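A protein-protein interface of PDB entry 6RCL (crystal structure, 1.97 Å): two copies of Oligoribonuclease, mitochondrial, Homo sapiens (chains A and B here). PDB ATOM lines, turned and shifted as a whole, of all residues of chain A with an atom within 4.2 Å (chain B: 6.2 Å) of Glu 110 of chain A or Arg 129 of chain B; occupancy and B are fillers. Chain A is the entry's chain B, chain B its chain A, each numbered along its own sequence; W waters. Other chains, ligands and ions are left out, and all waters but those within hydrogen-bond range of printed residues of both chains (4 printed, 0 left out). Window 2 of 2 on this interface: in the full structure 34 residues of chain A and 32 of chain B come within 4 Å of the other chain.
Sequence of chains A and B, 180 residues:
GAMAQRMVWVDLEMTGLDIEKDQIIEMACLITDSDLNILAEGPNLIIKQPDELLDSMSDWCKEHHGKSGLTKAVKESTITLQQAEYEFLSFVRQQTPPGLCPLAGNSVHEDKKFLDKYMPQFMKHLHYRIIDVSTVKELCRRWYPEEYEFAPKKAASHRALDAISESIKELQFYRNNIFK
The backbone carbonyl oxygen of Leu 103 of chain B sits at hydrogen-bond distance from the backbone NH of Ile 131 of chain B (3.0 Å). The side-chain hydroxyl of Ser 107 of chain A sits at hydrogen-bond distance from the side-chain hydroxyl of Ser 134 of chain A, 2.9 Å away. The backbone NH (N) of Arg 129 of chain B lies close to a ring nitrogen (ND1) of His 127 of chain B (3.4 Å).
The guanidinium group (NH1) of Arg 129 of chain B is in salt-bridge range of the side-chain carboxylate (OE2) of Glu 110 of chain A (3.9 Å). NE2 of His 109 of chain A is in hydrogen-bond range of O of Tyr 128 of chain B, at 3.4 Å.
1 position is printed for both chains. Of the 7 pairs that touch across the chains among the printed residues, none has its exchanged pair printed and touching as well.
Among the printed residues, merely in contact across the chains: His 109 of chain A with Ile 130 of chain B (3.6 Å), Ser 107 of chain A with Arg 129 of chain B (3.6 Å), Glu 138 of chain A with Arg 129 of chain B (3.7 Å), Ser 134 of chain A with Arg 129 of chain B (3.9 Å) and Glu 138 of chain A with Ile 131 of chain B (3.9 Å).
Of chain B, only Arg 129 (3.9 Å) comes within 4 Å of Glu 110 of chain A. Arg 129 of chain B touches just these residues of chain A: Ser 107 (3.6 Å), Glu 110 (3.9 Å), Ser 134 (3.9 Å) and Glu 138 (3.7 Å). Printed residues of chain B within 4 Å of Ser 107 of chain A: Arg 129. Of the printed residues of chain B, Ser 134 of chain A touches Arg 129 (3.9 Å). Lys 112 of chain A touches none of the printed residues of chain B. Lys 112 of chain B touches none of the printed residues of chain A. The nearest printed residue of chain A that does not touch Arg 129 of chain B is His 109 of chain A (4.6 Å). The nearest printed residue of chain B that does not touch Glu 138 of chain A is Ile 130 of chain B (4.4 Å).
Water W1 lies within hydrogen-bond range of the side-chain carboxylate (OE2) of Glu 110 of chain A, the backbone carbonyl oxygen (O) of Tyr 128 of chain B and a ring nitrogen (NE2) of His 109 of chain A. Water W2 bridges the side-chain hydroxyl of Ser 134 of chain A (2.7 Å) and the backbone carbonyl oxygen of Ile 130 of chain B (2.8 Å). Water W3 bridges the side-chain amino group (NZ) of Lys 112 of chain B and the backbone carbonyl oxygen (O) of His 109 of chain A. Water W4 bridges ND1 of His 127 of chain B (3.0 Å) and OE2 of Glu 138 of chain A (3.1 Å).
Of the 10 printed residues of chain B, 4 touch a printed residue of chain A. Hydrophobic or aromatic side chains of chain B that line the printed part of chain A: Ile 130 and Ile 131. Hydrophobic or aromatic side chains of chain A that line the printed part of chain B: His 109. Among the printed residues, Asp or Glu carboxylates within 4 Å of a Lys or Arg side-chain nitrogen of the other chain: Glu 110 of chain A with Arg 129 of chain B.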
ATOM      1  N   LEU A  17      25.461 -14.768 -20.753  1.00  0.00           N
ATOM      2  CA  LEU A  17      24.868 -16.108 -20.648  1.00  0.00           C
ATOM      3  C   LEU A  17      25.872 -17.251 -20.324  1.00  0.00           C
ATOM      4  O   LEU A  17      25.434 -18.397 -20.205  1.00  0.00           O
ATOM      5  CB  LEU A  17      24.081 -16.427 -21.935  1.00  0.00           C
ATOM      6  CG  LEU A  17      22.961 -15.439 -22.309  1.00  0.00           C
ATOM      7  CD1 LEU A  17      22.403 -15.753 -23.690  1.00  0.00           C
ATOM      8  CD2 LEU A  17      21.831 -15.441 -21.269  1.00  0.00           C
ATOM      9  N   SER A 107      11.751 -15.737 -20.268  1.00  0.00           N
ATOM     10  CA  SER A 107      13.002 -16.539 -20.434  1.00  0.00           C
ATOM     11  C   SER A 107      13.662 -16.847 -19.031  1.00  0.00           C
ATOM     12  O   SER A 107      14.863 -16.683 -18.824  1.00  0.00           O
ATOM     13  CB  SER A 107      13.971 -15.846 -21.393  1.00  0.00           C
ATOM     14  OG  SER A 107      13.559 -16.108 -22.722  1.00  0.00           O
ATOM     15  N   VAL A 108      12.824 -17.289 -18.078  1.00  0.00           N
ATOM     16  CA  VAL A 108      13.247 -17.571 -16.716  1.00  0.00           C
ATOM     17  C   VAL A 108      14.125 -18.852 -16.649  1.00  0.00           C
ATOM     18  O   VAL A 108      14.717 -19.120 -15.608  1.00  0.00           O
ATOM     19  CB  VAL A 108      12.018 -17.578 -15.760  1.00  0.00           C
ATOM     20  CG1 VAL A 108      11.294 -18.916 -15.762  1.00  0.00           C
ATOM     21  CG2 VAL A 108      12.395 -17.151 -14.350  1.00  0.00           C
ATOM     22  N   HIS A 109      14.216 -19.640 -17.750  1.00  0.00           N
ATOM     23  CA  HIS A 109      15.137 -20.788 -17.791  1.00  0.00           C
ATOM     24  C   HIS A 109      16.594 -20.266 -17.708  1.00  0.00           C
ATOM     25  O   HIS A 109      17.432 -20.897 -17.060  1.00  0.00           O
ATOM     26  CB  HIS A 109      14.948 -21.643 -19.048  1.00  0.00           C
ATOM     27  CG  HIS A 109      15.102 -20.895 -20.334  1.00  0.00           C
ATOM     28  ND1 HIS A 109      14.036 -20.231 -20.913  1.00  0.00           N
ATOM     29  CD2 HIS A 109      16.186 -20.758 -21.133  1.00  0.00           C
ATOM     30  CE1 HIS A 109      14.516 -19.654 -22.001  1.00  0.00           C
ATOM     31  NE2 HIS A 109      15.796 -19.973 -22.193  1.00  0.00           N
ATOM     32  N   GLU A 110      16.868 -19.093 -18.327  1.00  0.00           N
ATOM     33  CA  GLU A 110      18.181 -18.442 -18.269  1.00  0.00           C
ATOM     34  C   GLU A 110      18.467 -18.045 -16.813  1.00  0.00           C
ATOM     35  O   GLU A 110      19.556 -18.313 -16.308  1.00  0.00           O
ATOM     36  CB  GLU A 110      18.226 -17.187 -19.170  1.00  0.00           C
ATOM     37  CG  GLU A 110      18.083 -17.461 -20.664  1.00  0.00           C
ATOM     38  CD  GLU A 110      17.929 -16.244 -21.567  1.00  0.00           C
ATOM     39  OE1 GLU A 110      17.732 -15.119 -21.052  1.00  0.00           O
ATOM     40  OE2 GLU A 110      17.997 -16.421 -22.805  1.00  0.00           O
ATOM     41  N   ASP A 111      17.467 -17.441 -16.137  1.00  0.00           N
ATOM     42  CA  ASP A 111      17.562 -17.006 -14.732  1.00  0.00           C
ATOM     43  C   ASP A 111      17.764 -18.195 -13.784  1.00  0.00           C
ATOM     44  O   ASP A 111      18.599 -18.115 -12.882  1.00  0.00           O
ATOM     45  CB  ASP A 111      16.292 -16.230 -14.304  1.00  0.00           C
ATOM     46  CG  ASP A 111      16.016 -14.933 -15.061  1.00  0.00           C
ATOM     47  OD1 ASP A 111      16.768 -14.620 -16.000  1.00  0.00           O
ATOM     48  OD2 ASP A 111      15.048 -14.239 -14.713  1.00  0.00           O
ATOM     49  N   LYS A 112      17.015 -19.301 -13.999  1.00  0.00           N
ATOM     50  CA  LYS A 112      17.118 -20.497 -13.157  1.00  0.00           C
ATOM     51  C   LYS A 112      18.543 -21.090 -13.164  1.00  0.00           C
ATOM     52  O   LYS A 112      19.042 -21.482 -12.114  1.00  0.00           O
ATOM     53  CB  LYS A 112      16.090 -21.555 -13.581  1.00  0.00           C
ATOM     54  CG  LYS A 112      16.146 -22.791 -12.719  1.00  0.00           C
ATOM     55  CD  LYS A 112      14.908 -23.624 -12.774  1.00  0.00           C
ATOM     56  CE  LYS A 112      14.946 -24.729 -11.761  1.00  0.00           C
ATOM     57  NZ  LYS A 112      16.009 -25.733 -12.021  1.00  0.00           N
ATOM     58  N   LYS A 113      19.196 -21.124 -14.329  1.00  0.00           N
ATOM     59  CA  LYS A 113      20.561 -21.655 -14.454  1.00  0.00           C
ATOM     60  C   LYS A 113      21.534 -20.907 -13.519  1.00  0.00           C
ATOM     61  O   LYS A 113      22.325 -21.548 -12.821  1.00  0.00           O
ATOM     62  CB  LYS A 113      21.043 -21.536 -15.908  1.00  0.00           C
ATOM     63  CG  LYS A 113      22.219 -22.420 -16.257  1.00  0.00           C
ATOM     64  CD  LYS A 113      22.605 -22.207 -17.715  1.00  0.00           C
ATOM     65  CE  LYS A 113      23.513 -23.284 -18.237  1.00  0.00           C
ATOM     66  NZ  LYS A 113      24.098 -22.897 -19.537  1.00  0.00           N
ATOM     67  N   PHE A 114      21.442 -19.561 -13.486  1.00  0.00           N
ATOM     68  CA  PHE A 114      22.293 -18.728 -12.627  1.00  0.00           C
ATOM     69  C   PHE A 114      21.883 -18.823 -11.146  1.00  0.00           C
ATOM     70  O   PHE A 114      22.764 -18.864 -10.293  1.00  0.00           O
ATOM     71  CB  PHE A 114      22.361 -17.270 -13.123  1.00  0.00           C
ATOM     72  CG  PHE A 114      23.265 -17.096 -14.329  1.00  0.00           C
ATOM     73  CD1 PHE A 114      22.843 -17.476 -15.595  1.00  0.00           C
ATOM     74  CD2 PHE A 114      24.553 -16.594 -14.188  1.00  0.00           C
ATOM     75  CE1 PHE A 114      23.693 -17.372 -16.697  1.00  0.00           C
ATOM     76  CE2 PHE A 114      25.399 -16.479 -15.295  1.00  0.00           C
ATOM     77  CZ  PHE A 114      24.961 -16.859 -16.543  1.00  0.00           C
ATOM     78  N   SER A 134       8.186 -16.752 -22.040  1.00  0.00           N
ATOM     79  CA  SER A 134       8.602 -16.788 -23.439  1.00  0.00           C
ATOM     80  C   SER A 134       8.257 -18.145 -24.136  1.00  0.00           C
ATOM     81  O   SER A 134       8.172 -18.183 -25.348  1.00  0.00           O
ATOM     82  CB  SER A 134      10.061 -16.387 -23.593  1.00  0.00           C
ATOM     83  OG  SER A 134      10.917 -17.369 -23.065  1.00  0.00           O
ATOM     84  N   GLU A 138       6.339 -18.200 -27.737  1.00  0.00           N
ATOM     85  CA  GLU A 138       6.685 -19.067 -28.875  1.00  0.00           C
ATOM     86  C   GLU A 138       5.461 -19.817 -29.404  1.00  0.00           C
ATOM     87  O   GLU A 138       5.371 -20.015 -30.602  1.00  0.00           O
ATOM     88  CB  GLU A 138       7.820 -20.050 -28.502  1.00  0.00           C
ATOM     89  CG  GLU A 138       9.194 -19.397 -28.409  1.00  0.00           C
ATOM     90  CD  GLU A 138       9.699 -18.716 -29.672  1.00  0.00           C
ATOM     91  OE1 GLU A 138      10.233 -17.589 -29.580  1.00  0.00           O
ATOM     92  OE2 GLU A 138       9.555 -19.310 -30.761  1.00  0.00           O
ATOM     93  N   CYS B 101      15.353 -22.647 -34.413  1.00  0.00           N
ATOM     94  CA  CYS B 101      14.352 -23.529 -33.809  1.00  0.00           C
ATOM     95  C   CYS B 101      14.626 -23.797 -32.340  1.00  0.00           C
ATOM     96  O   CYS B 101      15.791 -24.001 -31.968  1.00  0.00           O
ATOM     97  CB  CYS B 101      14.268 -24.822 -34.600  1.00  0.00           C
ATOM     98  SG  CYS B 101      13.696 -24.561 -36.284  1.00  0.00           S
ATOM     99  N   PRO B 102      13.575 -23.817 -31.488  1.00  0.00           N
ATOM    100  CA  PRO B 102      13.805 -24.032 -30.048  1.00  0.00           C
ATOM    101  C   PRO B 102      13.880 -25.491 -29.640  1.00  0.00           C
ATOM    102  O   PRO B 102      13.216 -26.347 -30.229  1.00  0.00           O
ATOM    103  CB  PRO B 102      12.565 -23.405 -29.411  1.00  0.00           C
ATOM    104  CG  PRO B 102      11.467 -23.686 -30.432  1.00  0.00           C
ATOM    105  CD  PRO B 102      12.148 -23.576 -31.770  1.00  0.00           C
ATOM    106  N   LEU B 103      14.574 -25.727 -28.528  1.00  0.00           N
ATOM    107  CA  LEU B 103      14.611 -27.009 -27.839  1.00  0.00           C
ATOM    108  C   LEU B 103      13.221 -27.159 -27.175  1.00  0.00           C
ATOM    109  O   LEU B 103      12.717 -26.200 -26.599  1.00  0.00           O
ATOM    110  CB  LEU B 103      15.694 -26.948 -26.749  1.00  0.00           C
ATOM    111  CG  LEU B 103      16.075 -28.236 -26.055  1.00  0.00           C
ATOM    112  CD1 LEU B 103      16.784 -29.204 -27.046  1.00  0.00           C
ATOM    113  CD2 LEU B 103      16.976 -27.922 -24.845  1.00  0.00           C
ATOM    114  N   LYS B 112      18.659 -28.750 -21.245  1.00  0.00           N
ATOM    115  CA  LYS B 112      19.488 -27.665 -21.811  1.00  0.00           C
ATOM    116  C   LYS B 112      20.757 -27.446 -20.971  1.00  0.00           C
ATOM    117  O   LYS B 112      21.805 -27.196 -21.548  1.00  0.00           O
ATOM    118  CB  LYS B 112      18.690 -26.354 -21.886  1.00  0.00           C
ATOM    119  CG  LYS B 112      19.413 -25.230 -22.611  1.00  0.00           C
ATOM    120  CD  LYS B 112      18.629 -23.901 -22.547  1.00  0.00           C
ATOM    121  CE  LYS B 112      19.486 -22.734 -22.989  1.00  0.00           C
ATOM    122  NZ  LYS B 112      20.406 -22.265 -21.911  1.00  0.00           N
ATOM    123  N   LEU B 126      20.449 -24.552 -32.290  1.00  0.00           N
ATOM    124  CA  LEU B 126      19.114 -24.166 -31.843  1.00  0.00           C
ATOM    125  C   LEU B 126      19.057 -22.695 -31.438  1.00  0.00           C
ATOM    126  O   LEU B 126      20.094 -22.087 -31.179  1.00  0.00           O
ATOM    127  CB  LEU B 126      18.734 -25.079 -30.645  1.00  0.00           C
ATOM    128  CG  LEU B 126      18.860 -26.579 -30.898  1.00  0.00           C
ATOM    129  CD1 LEU B 126      18.354 -27.352 -29.716  1.00  0.00           C
ATOM    130  CD2 LEU B 126      18.069 -27.011 -32.130  1.00  0.00           C
ATOM    131  N   HIS B 127      17.840 -22.123 -31.367  1.00  0.00           N
ATOM    132  CA  HIS B 127      17.645 -20.734 -30.919  1.00  0.00           C
ATOM    133  C   HIS B 127      17.864 -20.676 -29.384  1.00  0.00           C
ATOM    134  O   HIS B 127      18.028 -21.714 -28.743  1.00  0.00           O
ATOM    135  CB  HIS B 127      16.215 -20.255 -31.242  1.00  0.00           C
ATOM    136  CG  HIS B 127      16.018 -18.764 -31.177  1.00  0.00           C
ATOM    137  ND1 HIS B 127      15.097 -18.200 -30.319  1.00  0.00           N
ATOM    138  CD2 HIS B 127      16.586 -17.776 -31.909  1.00  0.00           C
ATOM    139  CE1 HIS B 127      15.213 -16.891 -30.466  1.00  0.00           C
ATOM    140  NE2 HIS B 127      16.070 -16.594 -31.446  1.00  0.00           N
ATOM    141  N   TYR B 128      17.850 -19.457 -28.830  1.00  0.00           N
ATOM    142  CA  TYR B 128      17.960 -19.159 -27.393  1.00  0.00           C
ATOM    143  C   TYR B 128      16.744 -19.640 -26.600  1.00  0.00           C
ATOM    144  O   TYR B 128      16.871 -20.064 -25.447  1.00  0.00           O
ATOM    145  CB  TYR B 128      18.057 -17.638 -27.183  1.00  0.00           C
ATOM    146  CG  TYR B 128      19.327 -17.071 -27.750  1.00  0.00           C
ATOM    147  CD1 TYR B 128      20.542 -17.272 -27.112  1.00  0.00           C
ATOM    148  CD2 TYR B 128      19.333 -16.399 -28.968  1.00  0.00           C
ATOM    149  CE1 TYR B 128      21.726 -16.763 -27.632  1.00  0.00           C
ATOM    150  CE2 TYR B 128      20.519 -15.924 -29.526  1.00  0.00           C
ATOM    151  CZ  TYR B 128      21.713 -16.096 -28.845  1.00  0.00           C
ATOM    152  OH  TYR B 128      22.881 -15.609 -29.377  1.00  0.00           O
ATOM    153  N   ARG B 129      15.569 -19.473 -27.190  1.00  0.00           N
ATOM    154  CA  ARG B 129      14.301 -19.803 -26.551  1.00  0.00           C
ATOM    155  C   ARG B 129      14.041 -21.290 -26.502  1.00  0.00           C
ATOM    156  O   ARG B 129      14.515 -22.034 -27.346  1.00  0.00           O
ATOM    157  CB  ARG B 129      13.131 -19.148 -27.302  1.00  0.00           C
ATOM    158  CG  ARG B 129      13.252 -17.625 -27.504  1.00  0.00           C
ATOM    159  CD  ARG B 129      13.042 -16.827 -26.253  1.00  0.00           C
ATOM    160  NE  ARG B 129      13.454 -15.430 -26.444  1.00  0.00           N
ATOM    161  CZ  ARG B 129      14.689 -14.946 -26.265  1.00  0.00           C
ATOM    162  NH1 ARG B 129      15.676 -15.741 -25.862  1.00  0.00           N
ATOM    163  NH2 ARG B 129      14.945 -13.660 -26.488  1.00  0.00           N
ATOM    164  N   ILE B 130      13.246 -21.710 -25.516  1.00  0.00           N
ATOM    165  CA  ILE B 130      12.788 -23.082 -25.364  1.00  0.00           C
ATOM    166  C   ILE B 130      11.256 -23.102 -25.379  1.00  0.00           C
ATOM    167  O   ILE B 130      10.586 -22.074 -25.181  1.00  0.00           O
ATOM    168  CB  ILE B 130      13.328 -23.775 -24.075  1.00  0.00           C
ATOM    169  CG1 ILE B 130      12.625 -23.232 -22.775  1.00  0.00           C
ATOM    170  CG2 ILE B 130      14.854 -23.646 -24.019  1.00  0.00           C
ATOM    171  CD1 ILE B 130      13.186 -23.742 -21.424  1.00  0.00           C
ATOM    172  N   ILE B 131      10.724 -24.303 -25.522  1.00  0.00           N
ATOM    173  CA  ILE B 131       9.297 -24.564 -25.422  1.00  0.00           C
ATOM    174  C   ILE B 131       9.201 -25.595 -24.315  1.00  0.00           C
ATOM    175  O   ILE B 131       9.506 -26.779 -24.509  1.00  0.00           O
ATOM    176  CB  ILE B 131       8.691 -25.013 -26.774  1.00  0.00           C
ATOM    177  CG1 ILE B 131       8.708 -23.769 -27.746  1.00  0.00           C
ATOM    178  CG2 ILE B 131       7.232 -25.559 -26.542  1.00  0.00           C
ATOM    179  CD1 ILE B 131       8.107 -23.974 -29.117  1.00  0.00           C
HETATM  180  O   HOH W   1      18.703 -18.900 -23.449  1.00  0.00           O
HETATM  181  O   HOH W   2      11.530 -19.844 -23.865  1.00  0.00           O
HETATM  182  O   HOH W   3      19.157 -21.995 -19.466  1.00  0.00           O
HETATM  183  O   HOH W   4      12.632 -19.712 -31.206  1.00  0.00           O
